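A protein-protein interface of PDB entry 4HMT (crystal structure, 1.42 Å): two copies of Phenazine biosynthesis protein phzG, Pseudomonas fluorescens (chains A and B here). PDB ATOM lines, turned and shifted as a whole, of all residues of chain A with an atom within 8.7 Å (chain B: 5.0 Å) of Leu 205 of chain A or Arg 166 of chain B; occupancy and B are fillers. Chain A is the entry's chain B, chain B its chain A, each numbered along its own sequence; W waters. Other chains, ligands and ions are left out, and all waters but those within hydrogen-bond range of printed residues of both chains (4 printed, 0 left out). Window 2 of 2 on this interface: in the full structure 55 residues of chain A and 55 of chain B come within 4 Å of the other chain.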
ATOM      1  N   PHE A  30      -8.332   0.305  27.898  1.00  0.00           N
ATOM      2  CA  PHE A  30      -9.755   0.577  27.703  1.00  0.00           C
ATOM      3  C   PHE A  30     -10.555  -0.230  28.722  1.00  0.00           C
ATOM      4  O   PHE A  30     -11.442  -1.012  28.376  1.00  0.00           O
ATOM      5  CB  PHE A  30     -10.120   0.227  26.279  1.00  0.00           C
ATOM      6  CG  PHE A  30     -11.441   0.746  25.770  1.00  0.00           C
ATOM      7  CD1 PHE A  30     -12.298   1.519  26.513  1.00  0.00           C
ATOM      8  CD2 PHE A  30     -11.808   0.455  24.454  1.00  0.00           C
ATOM      9  CE1 PHE A  30     -13.502   1.966  25.983  1.00  0.00           C
ATOM     10  CE2 PHE A  30     -13.019   0.881  23.936  1.00  0.00           C
ATOM     11  CZ  PHE A  30     -13.843   1.673  24.666  1.00  0.00           C
ATOM     12  N   TYR A  33     -14.504  -0.376  28.507  1.00  0.00           N
ATOM     13  CA  TYR A  33     -15.237  -1.362  27.703  1.00  0.00           C
ATOM     14  C   TYR A  33     -15.724  -2.525  28.578  1.00  0.00           C
ATOM     15  O   TYR A  33     -16.766  -3.124  28.268  1.00  0.00           O
ATOM     16  CB  TYR A  33     -14.373  -1.849  26.551  1.00  0.00           C
ATOM     17  CG  TYR A  33     -15.043  -2.785  25.579  1.00  0.00           C
ATOM     18  CD1 TYR A  33     -15.999  -2.328  24.643  1.00  0.00           C
ATOM     19  CD2 TYR A  33     -14.761  -4.149  25.604  1.00  0.00           C
ATOM     20  CE1 TYR A  33     -16.571  -3.190  23.682  1.00  0.00           C
ATOM     21  CE2 TYR A  33     -15.368  -5.008  24.678  1.00  0.00           C
ATOM     22  CZ  TYR A  33     -16.261  -4.515  23.730  1.00  0.00           C
ATOM     23  OH  TYR A  33     -16.808  -5.370  22.813  1.00  0.00           O
ATOM     24  N   GLN A  34     -14.969  -2.818  29.619  1.00  0.00           N
ATOM     25  CA  GLN A  34     -15.354  -3.879  30.550  1.00  0.00           C
ATOM     26  C   GLN A  34     -16.329  -3.373  31.627  1.00  0.00           C
ATOM     27  O   GLN A  34     -17.274  -4.065  32.012  1.00  0.00           O
ATOM     28  CB  GLN A  34     -14.136  -4.453  31.254  1.00  0.00           C
ATOM     29  CG  GLN A  34     -12.968  -4.883  30.336  1.00  0.00           C
ATOM     30  CD  GLN A  34     -13.378  -5.830  29.308  1.00  0.00           C
ATOM     31  OE1 GLN A  34     -14.224  -6.710  29.553  1.00  0.00           O
ATOM     32  NE2 GLN A  34     -12.769  -5.701  28.117  1.00  0.00           N
ATOM     33  N   TRP A 198     -13.971   3.971  20.474  1.00  0.00           N
ATOM     34  CA  TRP A 198     -13.513   2.856  19.672  1.00  0.00           C
ATOM     35  C   TRP A 198     -12.055   2.575  19.979  1.00  0.00           C
ATOM     36  O   TRP A 198     -11.193   3.470  19.865  1.00  0.00           O
ATOM     37  CB  TRP A 198     -13.662   3.233  18.207  1.00  0.00           C
ATOM     38  CG  TRP A 198     -13.406   2.145  17.161  1.00  0.00           C
ATOM     39  CD1 TRP A 198     -14.362   1.503  16.460  1.00  0.00           C
ATOM     40  CD2 TRP A 198     -12.147   1.614  16.697  1.00  0.00           C
ATOM     41  NE1 TRP A 198     -13.823   0.614  15.575  1.00  0.00           N
ATOM     42  CE2 TRP A 198     -12.453   0.670  15.694  1.00  0.00           C
ATOM     43  CE3 TRP A 198     -10.798   1.881  16.983  1.00  0.00           C
ATOM     44  CZ2 TRP A 198     -11.484  -0.038  15.026  1.00  0.00           C
ATOM     45  CZ3 TRP A 198      -9.830   1.160  16.315  1.00  0.00           C
ATOM     46  CH2 TRP A 198     -10.181   0.217  15.334  1.00  0.00           C
ATOM     47  N   GLY A 199     -11.766   1.321  20.296  1.00  0.00           N
ATOM     48  CA  GLY A 199     -10.388   0.856  20.457  1.00  0.00           C
ATOM     49  C   GLY A 199     -10.126  -0.374  19.639  1.00  0.00           C
ATOM     50  O   GLY A 199     -11.034  -1.115  19.268  1.00  0.00           O
ATOM     51  N   ASN A 200      -8.857  -0.616  19.367  1.00  0.00           N
ATOM     52  CA  ASN A 200      -8.461  -1.700  18.473  1.00  0.00           C
ATOM     53  C   ASN A 200      -8.831  -3.070  19.035  1.00  0.00           C
ATOM     54  O   ASN A 200      -9.157  -3.989  18.288  1.00  0.00           O
ATOM     55  CB  ASN A 200      -6.969  -1.589  18.174  1.00  0.00           C
ATOM     56  CG  ASN A 200      -6.542  -2.524  17.102  1.00  0.00           C
ATOM     57  OD1 ASN A 200      -7.263  -2.784  16.121  1.00  0.00           O
ATOM     58  ND2 ASN A 200      -5.365  -3.040  17.274  1.00  0.00           N
ATOM     59  N   GLY A 201      -8.768  -3.211  20.331  1.00  0.00           N
ATOM     60  CA  GLY A 201      -9.099  -4.508  20.906  1.00  0.00           C
ATOM     61  C   GLY A 201      -8.086  -5.565  20.617  1.00  0.00           C
ATOM     62  O   GLY A 201      -6.969  -5.287  20.271  1.00  0.00           O
ATOM     63  N   GLN A 202      -8.513  -6.795  20.830  1.00  0.00           N
ATOM     64  CA  GLN A 202      -7.681  -7.990  20.634  1.00  0.00           C
ATOM     65  C   GLN A 202      -8.299  -8.833  19.507  1.00  0.00           C
ATOM     66  O   GLN A 202      -9.522  -8.966  19.450  1.00  0.00           O
ATOM     67  CB  GLN A 202      -7.614  -8.790  21.941  1.00  0.00           C
ATOM     68  CG  GLN A 202      -6.961  -8.037  23.072  1.00  0.00           C
ATOM     69  CD  GLN A 202      -7.388  -8.533  24.482  1.00  0.00           C
ATOM     70  OE1 GLN A 202      -8.082  -9.555  24.653  1.00  0.00           O
ATOM     71  NE2 GLN A 202      -6.985  -7.781  25.493  1.00  0.00           N
ATOM     72  N   GLU A 203      -7.456  -9.443  18.663  1.00  0.00           N
ATOM     73  CA  GLU A 203      -7.933 -10.366  17.630  1.00  0.00           C
ATOM     74  C   GLU A 203      -8.958  -9.753  16.680  1.00  0.00           C
ATOM     75  O   GLU A 203      -9.844 -10.438  16.200  1.00  0.00           O
ATOM     76  CB  GLU A 203      -8.569 -11.615  18.250  1.00  0.00           C
ATOM     77  CG  GLU A 203      -7.704 -12.313  19.275  1.00  0.00           C
ATOM     78  CD  GLU A 203      -8.483 -13.407  20.022  1.00  0.00           C
ATOM     79  OE1 GLU A 203      -8.810 -13.222  21.219  1.00  0.00           O
ATOM     80  OE2 GLU A 203      -8.779 -14.460  19.435  1.00  0.00           O
ATOM     81  N   ARG A 204      -8.829  -8.460  16.450  1.00  0.00           N
ATOM     82  CA  ARG A 204      -9.687  -7.696  15.536  1.00  0.00           C
ATOM     83  C   ARG A 204     -11.122  -7.604  16.056  1.00  0.00           C
ATOM     84  O   ARG A 204     -12.002  -7.038  15.344  1.00  0.00           O
ATOM     85  CB  ARG A 204      -9.656  -8.263  14.100  1.00  0.00           C
ATOM     86  CG  ARG A 204      -8.355  -8.063  13.461  1.00  0.00           C
ATOM     87  CD  ARG A 204      -8.195  -8.795  12.157  1.00  0.00           C
ATOM     88  NE  ARG A 204      -6.815  -8.697  11.643  1.00  0.00           N
ATOM     89  CZ  ARG A 204      -5.803  -9.532  11.908  1.00  0.00           C
ATOM     90  NH1 ARG A 204      -5.956 -10.591  12.682  1.00  0.00           N
ATOM     91  NH2 ARG A 204      -4.614  -9.285  11.380  1.00  0.00           N
ATOM     92  N   LEU A 205     -11.328  -7.958  17.336  1.00  0.00           N
ATOM     93  CA  LEU A 205     -12.620  -7.663  17.971  1.00  0.00           C
ATOM     94  C   LEU A 205     -12.496  -6.256  18.454  1.00  0.00           C
ATOM     95  O   LEU A 205     -12.254  -5.995  19.622  1.00  0.00           O
ATOM     96  CB  LEU A 205     -12.969  -8.654  19.075  1.00  0.00           C
ATOM     97  CG  LEU A 205     -14.466  -8.819  19.242  1.00  0.00           C
ATOM     98  CD1 LEU A 205     -14.791 -10.005  20.135  1.00  0.00           C
ATOM     99  CD2 LEU A 205     -15.101  -7.582  19.812  1.00  0.00           C
ATOM    100  N   HIS A 206     -12.678  -5.321  17.543  1.00  0.00           N
ATOM    101  CA  HIS A 206     -12.554  -3.917  17.922  1.00  0.00           C
ATOM    102  C   HIS A 206     -13.636  -3.566  18.944  1.00  0.00           C
ATOM    103  O   HIS A 206     -14.751  -4.073  18.904  1.00  0.00           O
ATOM    104  CB  HIS A 206     -12.673  -3.019  16.719  1.00  0.00           C
ATOM    105  CG  HIS A 206     -11.804  -3.411  15.592  1.00  0.00           C
ATOM    106  ND1 HIS A 206     -10.459  -3.611  15.753  1.00  0.00           N
ATOM    107  CD2 HIS A 206     -12.082  -3.634  14.282  1.00  0.00           C
ATOM    108  CE1 HIS A 206      -9.937  -3.976  14.591  1.00  0.00           C
ATOM    109  NE2 HIS A 206     -10.904  -4.010  13.686  1.00  0.00           N
ATOM    110  N   GLU A 207     -13.222  -2.773  19.897  1.00  0.00           N
ATOM    111  CA  GLU A 207     -13.989  -2.465  21.104  1.00  0.00           C
ATOM    112  C   GLU A 207     -14.739  -1.165  20.967  1.00  0.00           C
ATOM    113  O   GLU A 207     -14.127  -0.123  20.822  1.00  0.00           O
ATOM    114  CB  GLU A 207     -13.105  -2.491  22.333  1.00  0.00           C
ATOM    115  CG  GLU A 207     -12.542  -3.875  22.552  1.00  0.00           C
ATOM    116  CD  GLU A 207     -11.512  -4.030  23.663  1.00  0.00           C
ATOM    117  OE1 GLU A 207     -11.073  -3.019  24.257  1.00  0.00           O
ATOM    118  OE2 GLU A 207     -11.171  -5.200  23.972  1.00  0.00           O
ATOM    119  N   ARG A 208     -16.074  -1.257  20.873  1.00  0.00           N
ATOM    120  CA  ARG A 208     -16.936  -0.116  20.555  1.00  0.00           C
ATOM    121  C   ARG A 208     -17.891   0.054  21.730  1.00  0.00           C
ATOM    122  O   ARG A 208     -18.739  -0.799  21.991  1.00  0.00           O
ATOM    123  CB  ARG A 208     -17.718  -0.406  19.284  1.00  0.00           C
ATOM    124  CG  ARG A 208     -16.878  -0.670  18.077  1.00  0.00           C
ATOM    125  CD  ARG A 208     -17.677  -0.845  16.848  1.00  0.00           C
ATOM    126  NE  ARG A 208     -18.415   0.386  16.524  1.00  0.00           N
ATOM    127  CZ  ARG A 208     -19.319   0.498  15.559  1.00  0.00           C
ATOM    128  NH1 ARG A 208     -19.634  -0.525  14.793  1.00  0.00           N
ATOM    129  NH2 ARG A 208     -19.889   1.672  15.298  1.00  0.00           N
ATOM    130  N   ARG A 222     -22.413  -2.061  24.055  1.00  0.00           N
ATOM    131  CA  ARG A 222     -21.270  -2.417  23.209  1.00  0.00           C
ATOM    132  C   ARG A 222     -21.792  -2.674  21.790  1.00  0.00           C
ATOM    133  O   ARG A 222     -22.922  -3.191  21.606  1.00  0.00           O
ATOM    134  CB  ARG A 222     -20.582  -3.692  23.699  1.00  0.00           C
ATOM    135  CG  ARG A 222     -20.016  -3.591  25.086  1.00  0.00           C
ATOM    136  CD  ARG A 222     -19.278  -4.856  25.528  1.00  0.00           C
ATOM    137  NE  ARG A 222     -18.781  -4.738  26.891  1.00  0.00           N
ATOM    138  CZ  ARG A 222     -19.401  -5.176  27.981  1.00  0.00           C
ATOM    139  NH1 ARG A 222     -20.554  -5.831  27.901  1.00  0.00           N
ATOM    140  NH2 ARG A 222     -18.837  -4.998  29.132  1.00  0.00           N
ATOM    141  N   LEU A 223     -21.009  -2.302  20.779  1.00  0.00           N
ATOM    142  CA  LEU A 223     -21.405  -2.521  19.383  1.00  0.00           C
ATOM    143  C   LEU A 223     -20.493  -3.526  18.705  1.00  0.00           C
ATOM    144  O   LEU A 223     -19.301  -3.592  18.988  1.00  0.00           O
ATOM    145  CB  LEU A 223     -21.399  -1.210  18.554  1.00  0.00           C
ATOM    146  CG  LEU A 223     -22.299  -0.079  19.097  1.00  0.00           C
ATOM    147  CD1 LEU A 223     -22.208   1.109  18.162  1.00  0.00           C
ATOM    148  CD2 LEU A 223     -23.727  -0.530  19.283  1.00  0.00           C
ATOM    149  N   GLN A 224     -21.038  -4.239  17.735  1.00  0.00           N
ATOM    150  CA  GLN A 224     -20.253  -5.181  16.963  1.00  0.00           C
ATOM    151  C   GLN A 224     -19.340  -4.425  15.992  1.00  0.00           C
ATOM    152  O   GLN A 224     -19.739  -3.437  15.393  1.00  0.00           O
ATOM    153  CB  GLN A 224     -21.186  -6.131  16.209  1.00  0.00           C
ATOM    154  CG  GLN A 224     -22.023  -6.979  17.166  1.00  0.00           C
ATOM    155  CD  GLN A 224     -22.867  -8.019  16.436  1.00  0.00           C
ATOM    156  OE1 GLN A 224     -22.400  -8.703  15.515  1.00  0.00           O
ATOM    157  NE2 GLN A 224     -24.109  -8.170  16.862  1.00  0.00           N
ATOM    158  N   PRO A 225     -18.088  -4.917  15.853  1.00  0.00           N
ATOM    159  CA  PRO A 225     -17.097  -4.207  15.055  1.00  0.00           C
ATOM    160  C   PRO A 225     -17.316  -4.176  13.583  1.00  0.00           C
ATOM    161  O   PRO A 225     -16.791  -3.238  12.942  1.00  0.00           O
ATOM    162  CB  PRO A 225     -15.806  -4.954  15.371  1.00  0.00           C
ATOM    163  CG  PRO A 225     -16.199  -6.251  15.807  1.00  0.00           C
ATOM    164  CD  PRO A 225     -17.540  -6.117  16.487  1.00  0.00           C
ATOM    165  OXT PRO A 225     -17.961  -5.054  13.003  1.00  0.00           O
ATOM    166  N   MET B 149     -13.446 -12.237  11.684  1.00  0.00           N
ATOM    167  CA  MET B 149     -14.240 -11.308  12.426  1.00  0.00           C
ATOM    168  C   MET B 149     -15.270 -10.640  11.514  1.00  0.00           C
ATOM    169  O   MET B 149     -16.397 -10.351  11.951  1.00  0.00           O
ATOM    170  CB  MET B 149     -13.343 -10.265  13.128  1.00  0.00           C
ATOM    171  CG  MET B 149     -14.115  -9.424  14.177  1.00  0.00           C
ATOM    172  SD  MET B 149     -14.778 -10.500  15.514  1.00  0.00           S
ATOM    173  CE  MET B 149     -13.275 -11.143  16.211  1.00  0.00           C
ATOM    174  N   LEU B 159     -23.718  -5.656  20.513  1.00  0.00           N
ATOM    175  CA  LEU B 159     -22.937  -6.858  20.828  1.00  0.00           C
ATOM    176  C   LEU B 159     -23.369  -7.326  22.213  1.00  0.00           C
ATOM    177  O   LEU B 159     -23.043  -6.708  23.218  1.00  0.00           O
ATOM    178  CB  LEU B 159     -21.439  -6.536  20.816  1.00  0.00           C
ATOM    179  CG  LEU B 159     -20.474  -7.680  21.167  1.00  0.00           C
ATOM    180  CD1 LEU B 159     -20.741  -8.965  20.450  1.00  0.00           C
ATOM    181  CD2 LEU B 159     -19.012  -7.215  20.971  1.00  0.00           C
ATOM    182  N   VAL B 162     -19.640 -10.716  24.195  1.00  0.00           N
ATOM    183  CA  VAL B 162     -18.296 -10.500  23.634  1.00  0.00           C
ATOM    184  C   VAL B 162     -17.554 -11.824  23.470  1.00  0.00           C
ATOM    185  O   VAL B 162     -17.008 -12.116  22.402  1.00  0.00           O
ATOM    186  CB  VAL B 162     -17.445  -9.549  24.534  1.00  0.00           C
ATOM    187  CG1 VAL B 162     -16.064  -9.366  23.926  1.00  0.00           C
ATOM    188  CG2 VAL B 162     -18.111  -8.155  24.688  1.00  0.00           C
ATOM    189  N   GLN B 163     -17.556 -12.659  24.503  1.00  0.00           N
ATOM    190  CA  GLN B 163     -16.828 -13.933  24.437  1.00  0.00           C
ATOM    191  C   GLN B 163     -17.385 -14.843  23.331  1.00  0.00           C
ATOM    192  O   GLN B 163     -16.635 -15.568  22.653  1.00  0.00           O
ATOM    193  CB  GLN B 163     -16.828 -14.640  25.792  1.00  0.00           C
ATOM    194  CG  GLN B 163     -15.876 -15.849  25.782  1.00  0.00           C
ATOM    195  CD  GLN B 163     -14.405 -15.422  25.728  1.00  0.00           C
ATOM    196  OE1 GLN B 163     -14.004 -14.455  26.382  1.00  0.00           O
ATOM    197  NE2 GLN B 163     -13.608 -16.123  24.937  1.00  0.00           N
ATOM    198  N   ALA B 164     -18.701 -14.880  23.169  1.00  0.00           N
ATOM    199  CA  ALA B 164     -19.279 -15.700  22.104  1.00  0.00           C
ATOM    200  C   ALA B 164     -18.799 -15.254  20.716  1.00  0.00           C
ATOM    201  O   ALA B 164     -18.495 -16.099  19.867  1.00  0.00           O
ATOM    202  CB  ALA B 164     -20.804 -15.648  22.173  1.00  0.00           C
ATOM    203  N   MET B 165     -18.692 -13.953  20.488  1.00  0.00           N
ATOM    204  CA  MET B 165     -18.192 -13.439  19.225  1.00  0.00           C
ATOM    205  C   MET B 165     -16.728 -13.838  19.062  1.00  0.00           C
ATOM    206  O   MET B 165     -16.318 -14.332  17.993  1.00  0.00           O
ATOM    207  CB  MET B 165     -18.384 -11.920  19.114  1.00  0.00           C
ATOM    208  CG  MET B 165     -17.781 -11.374  17.858  1.00  0.00           C
ATOM    209  SD  MET B 165     -18.097  -9.687  17.527  1.00  0.00           S
ATOM    210  CE  MET B 165     -19.658  -9.846  16.864  1.00  0.00           C
ATOM    211  N   ARG B 166     -15.934 -13.665  20.111  1.00  0.00           N
ATOM    212  CA  ARG B 166     -14.515 -13.953  20.052  1.00  0.00           C
ATOM    213  C   ARG B 166     -14.320 -15.442  19.720  1.00  0.00           C
ATOM    214  O   ARG B 166     -13.523 -15.815  18.851  1.00  0.00           O
ATOM    215  CB  ARG B 166     -13.851 -13.602  21.377  1.00  0.00           C
ATOM    216  CG  ARG B 166     -12.355 -13.752  21.333  1.00  0.00           C
ATOM    217  CD  ARG B 166     -11.714 -13.307  22.657  1.00  0.00           C
ATOM    218  NE  ARG B 166     -12.022 -11.905  23.029  1.00  0.00           N
ATOM    219  CZ  ARG B 166     -11.553 -10.822  22.394  1.00  0.00           C
ATOM    220  NH1 ARG B 166     -10.792 -10.907  21.299  1.00  0.00           N
ATOM    221  NH2 ARG B 166     -11.897  -9.648  22.850  1.00  0.00           N
ATOM    222  N   ASN B 167     -15.110 -16.300  20.365  1.00  0.00           N
ATOM    223  CA  ASN B 167     -14.936 -17.738  20.184  1.00  0.00           C
ATOM    224  C   ASN B 167     -15.396 -18.179  18.785  1.00  0.00           C
ATOM    225  O   ASN B 167     -14.769 -19.058  18.167  1.00  0.00           O
ATOM    226  CB  ASN B 167     -15.680 -18.527  21.259  1.00  0.00           C
ATOM    227  CG  ASN B 167     -15.079 -18.402  22.604  1.00  0.00           C
ATOM    228  OD1 ASN B 167     -14.020 -17.858  22.769  1.00  0.00           O
ATOM    229  ND2 ASN B 167     -15.745 -18.962  23.591  1.00  0.00           N
ATOM    230  N   ALA B 168     -16.475 -17.588  18.263  1.00  0.00           N
ATOM    231  CA  ALA B 168     -16.933 -17.929  16.926  1.00  0.00           C
ATOM    232  C   ALA B 168     -15.872 -17.553  15.864  1.00  0.00           C
ATOM    233  O   ALA B 168     -15.601 -18.305  14.925  1.00  0.00           O
ATOM    234  CB  ALA B 168     -18.277 -17.249  16.611  1.00  0.00           C
ATOM    235  N   ALA B 169     -15.288 -16.377  16.011  1.00  0.00           N
ATOM    236  CA  ALA B 169     -14.240 -15.929  15.094  1.00  0.00           C
ATOM    237  C   ALA B 169     -13.009 -16.818  15.210  1.00  0.00           C
ATOM    238  O   ALA B 169     -12.413 -17.124  14.199  1.00  0.00           O
ATOM    239  CB  ALA B 169     -13.858 -14.447  15.357  1.00  0.00           C
ATOM    240  N   ARG B 170     -12.633 -17.229  16.424  1.00  0.00           N
ATOM    241  CA  ARG B 170     -11.490 -18.142  16.604  1.00  0.00           C
ATOM    242  C   ARG B 170     -11.733 -19.435  15.846  1.00  0.00           C
ATOM    243  O   ARG B 170     -10.803 -20.027  15.274  1.00  0.00           O
ATOM    244  CB  ARG B 170     -11.280 -18.435  18.097  1.00  0.00           C
ATOM    245  CG  ARG B 170     -10.544 -17.359  18.805  1.00  0.00           C
ATOM    246  CD  ARG B 170     -10.494 -17.576  20.347  1.00  0.00           C
ATOM    247  NE  ARG B 170      -9.804 -16.482  21.016  1.00  0.00           N
ATOM    248  CZ  ARG B 170      -9.625 -16.422  22.328  1.00  0.00           C
ATOM    249  NH1 ARG B 170     -10.072 -17.415  23.084  1.00  0.00           N
ATOM    250  NH2 ARG B 170      -8.968 -15.398  22.874  1.00  0.00           N
HETATM  251  O   HOH W   1     -11.195  -7.057  21.915  1.00  0.00           O
HETATM  252  O   HOH W   2     -24.221  -4.161  24.945  1.00  0.00           O
HETATM  253  O   HOH W   3     -22.147  -6.940  25.812  1.00  0.00           O
HETATM  254  O   HOH W   4     -11.316 -14.176  18.060  1.00  0.00           O
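O of Tyr 33 of chain A is in hydrogen-bond range of NH2 of Arg 222 of chain A (2.9 Å).
The guanidinium group (NH1) of Arg 208 of chain A lies within hydrogen-bond range of the backbone carbonyl oxygen (O) of Gln 224 of chain A, 3.0 Å away.
The backbone carbonyl oxygen (O) of Arg 208 of chain A lies within hydrogen-bond range of the backbone NH (N) of Leu 223 of chain A (3.0 Å).
O of Gln 34 of chain A is in hydrogen-bond range of NH2 of Arg 222 of chain A (3.4 Å).
No position is printed for both chains.
Water W1 lies within hydrogen-bond range of O of Leu 205 of chain A, OE2 of Glu 207 of chain A, NH2 of Arg 166 of chain B and N of Gln 202 of chain A.
Water W3 lies within hydrogen-bond range of the backbone carbonyl oxygen (O) of Leu 159 of chain B (2.8 Å) and the guanidinium group (NH1) of Arg 222 of chain A (2.9 Å).
Water W4 bridges the backbone carbonyl oxygen (O) of Arg 166 of chain B (2.9 Å) and the side-chain carboxylate (OE2) of Glu 203 of chain A (2.9 Å).
Water W2 bridges the backbone NH of Arg 222 of chain A (2.9 Å) and the backbone carbonyl oxygen of Leu 159 of chain B (3.3 Å).
Printed residues of chain B that touch a printed residue of chain A: Met 149, Leu 159, Val 162, Met 165, Arg 166 and Arg 170.
Of the 18 printed residues of chain A, 9 touch a printed residue of chain B.
Printed residues of chain A that touch a printed residue of chain B: Tyr 33, Gln 202, Glu 203, Arg 204, Leu 205, Arg 222, Leu 223, Gln 224 and Pro 225.
Hydrophobic or aromatic side chains of chain A that line the printed part of chain B: Tyr 33, Leu 205 and Pro 225.
The guanidinium group (NH1) of Arg 166 of chain B lies within hydrogen-bond range of the backbone carbonyl oxygen (O) of Gln 202 of chain A, 3.0 Å away.
OE1 of Glu 203 of chain A lies within salt-bridge range of NH2 of Arg 170 of chain B, at 2.7 Å.
The side-chain carboxylate (OE1) of Glu 203 of chain A is in salt-bridge range of the guanidinium group (NH1) of Arg 166 of chain B (3.0 Å).
The backbone carbonyl oxygen (O) of Arg 222 of chain A lies within hydrogen-bond range of the backbone NH (N) of Leu 159 of chain B (2.8 Å).
Of the printed residues of chain B, Leu 205 of chain A touches Met 149 (3.8 Å), Val 162 (3.8 Å), Met 165 (3.9999 Å) and Arg 166 (3.8 Å).
Of the printed residues of chain A, Met 149 of chain B touches Glu 203, Arg 204 and Leu 205.
Of the printed residues of chain B, Arg 222 of chain A touches Leu 159 and Val 162.
Of the printed residues of chain B, Arg 204 of chain A touches Met 149.
Printed residues of chain B within 4 Å of Leu 223 of chain A: Leu 159.
Ala 164 of chain B touches none of the printed residues of chain A.
Ala 168 of chain B touches none of the printed residues of chain A.
Tyr 33 of chain A touches Leu 159 of chain B.
O of Arg 204 of chain A touches CG of Met 149 of chain B (3.4 Å).
Leu 205 of chain A touches Met 149 of chain B (CB to CE, 3.8 Å).
Leu 205 of chain A touches Val 162 of chain B.
N of Arg 166 of chain B touches CD1 of Leu 205 of chain A, 3.8 Å away.
CG2 of Val 162 of chain B touches CD of Arg 222 of chain A, 3.6 Å away.
Leu 159 of chain B touches Leu 223 of chain A (CB to C, 3.8 Å).
Leu 159 of chain B touches Gln 224 of chain A.
Gln 224 of chain A touches Met 165 of chain B.
Pro 225 of chain A touches Met 165 of chain B.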
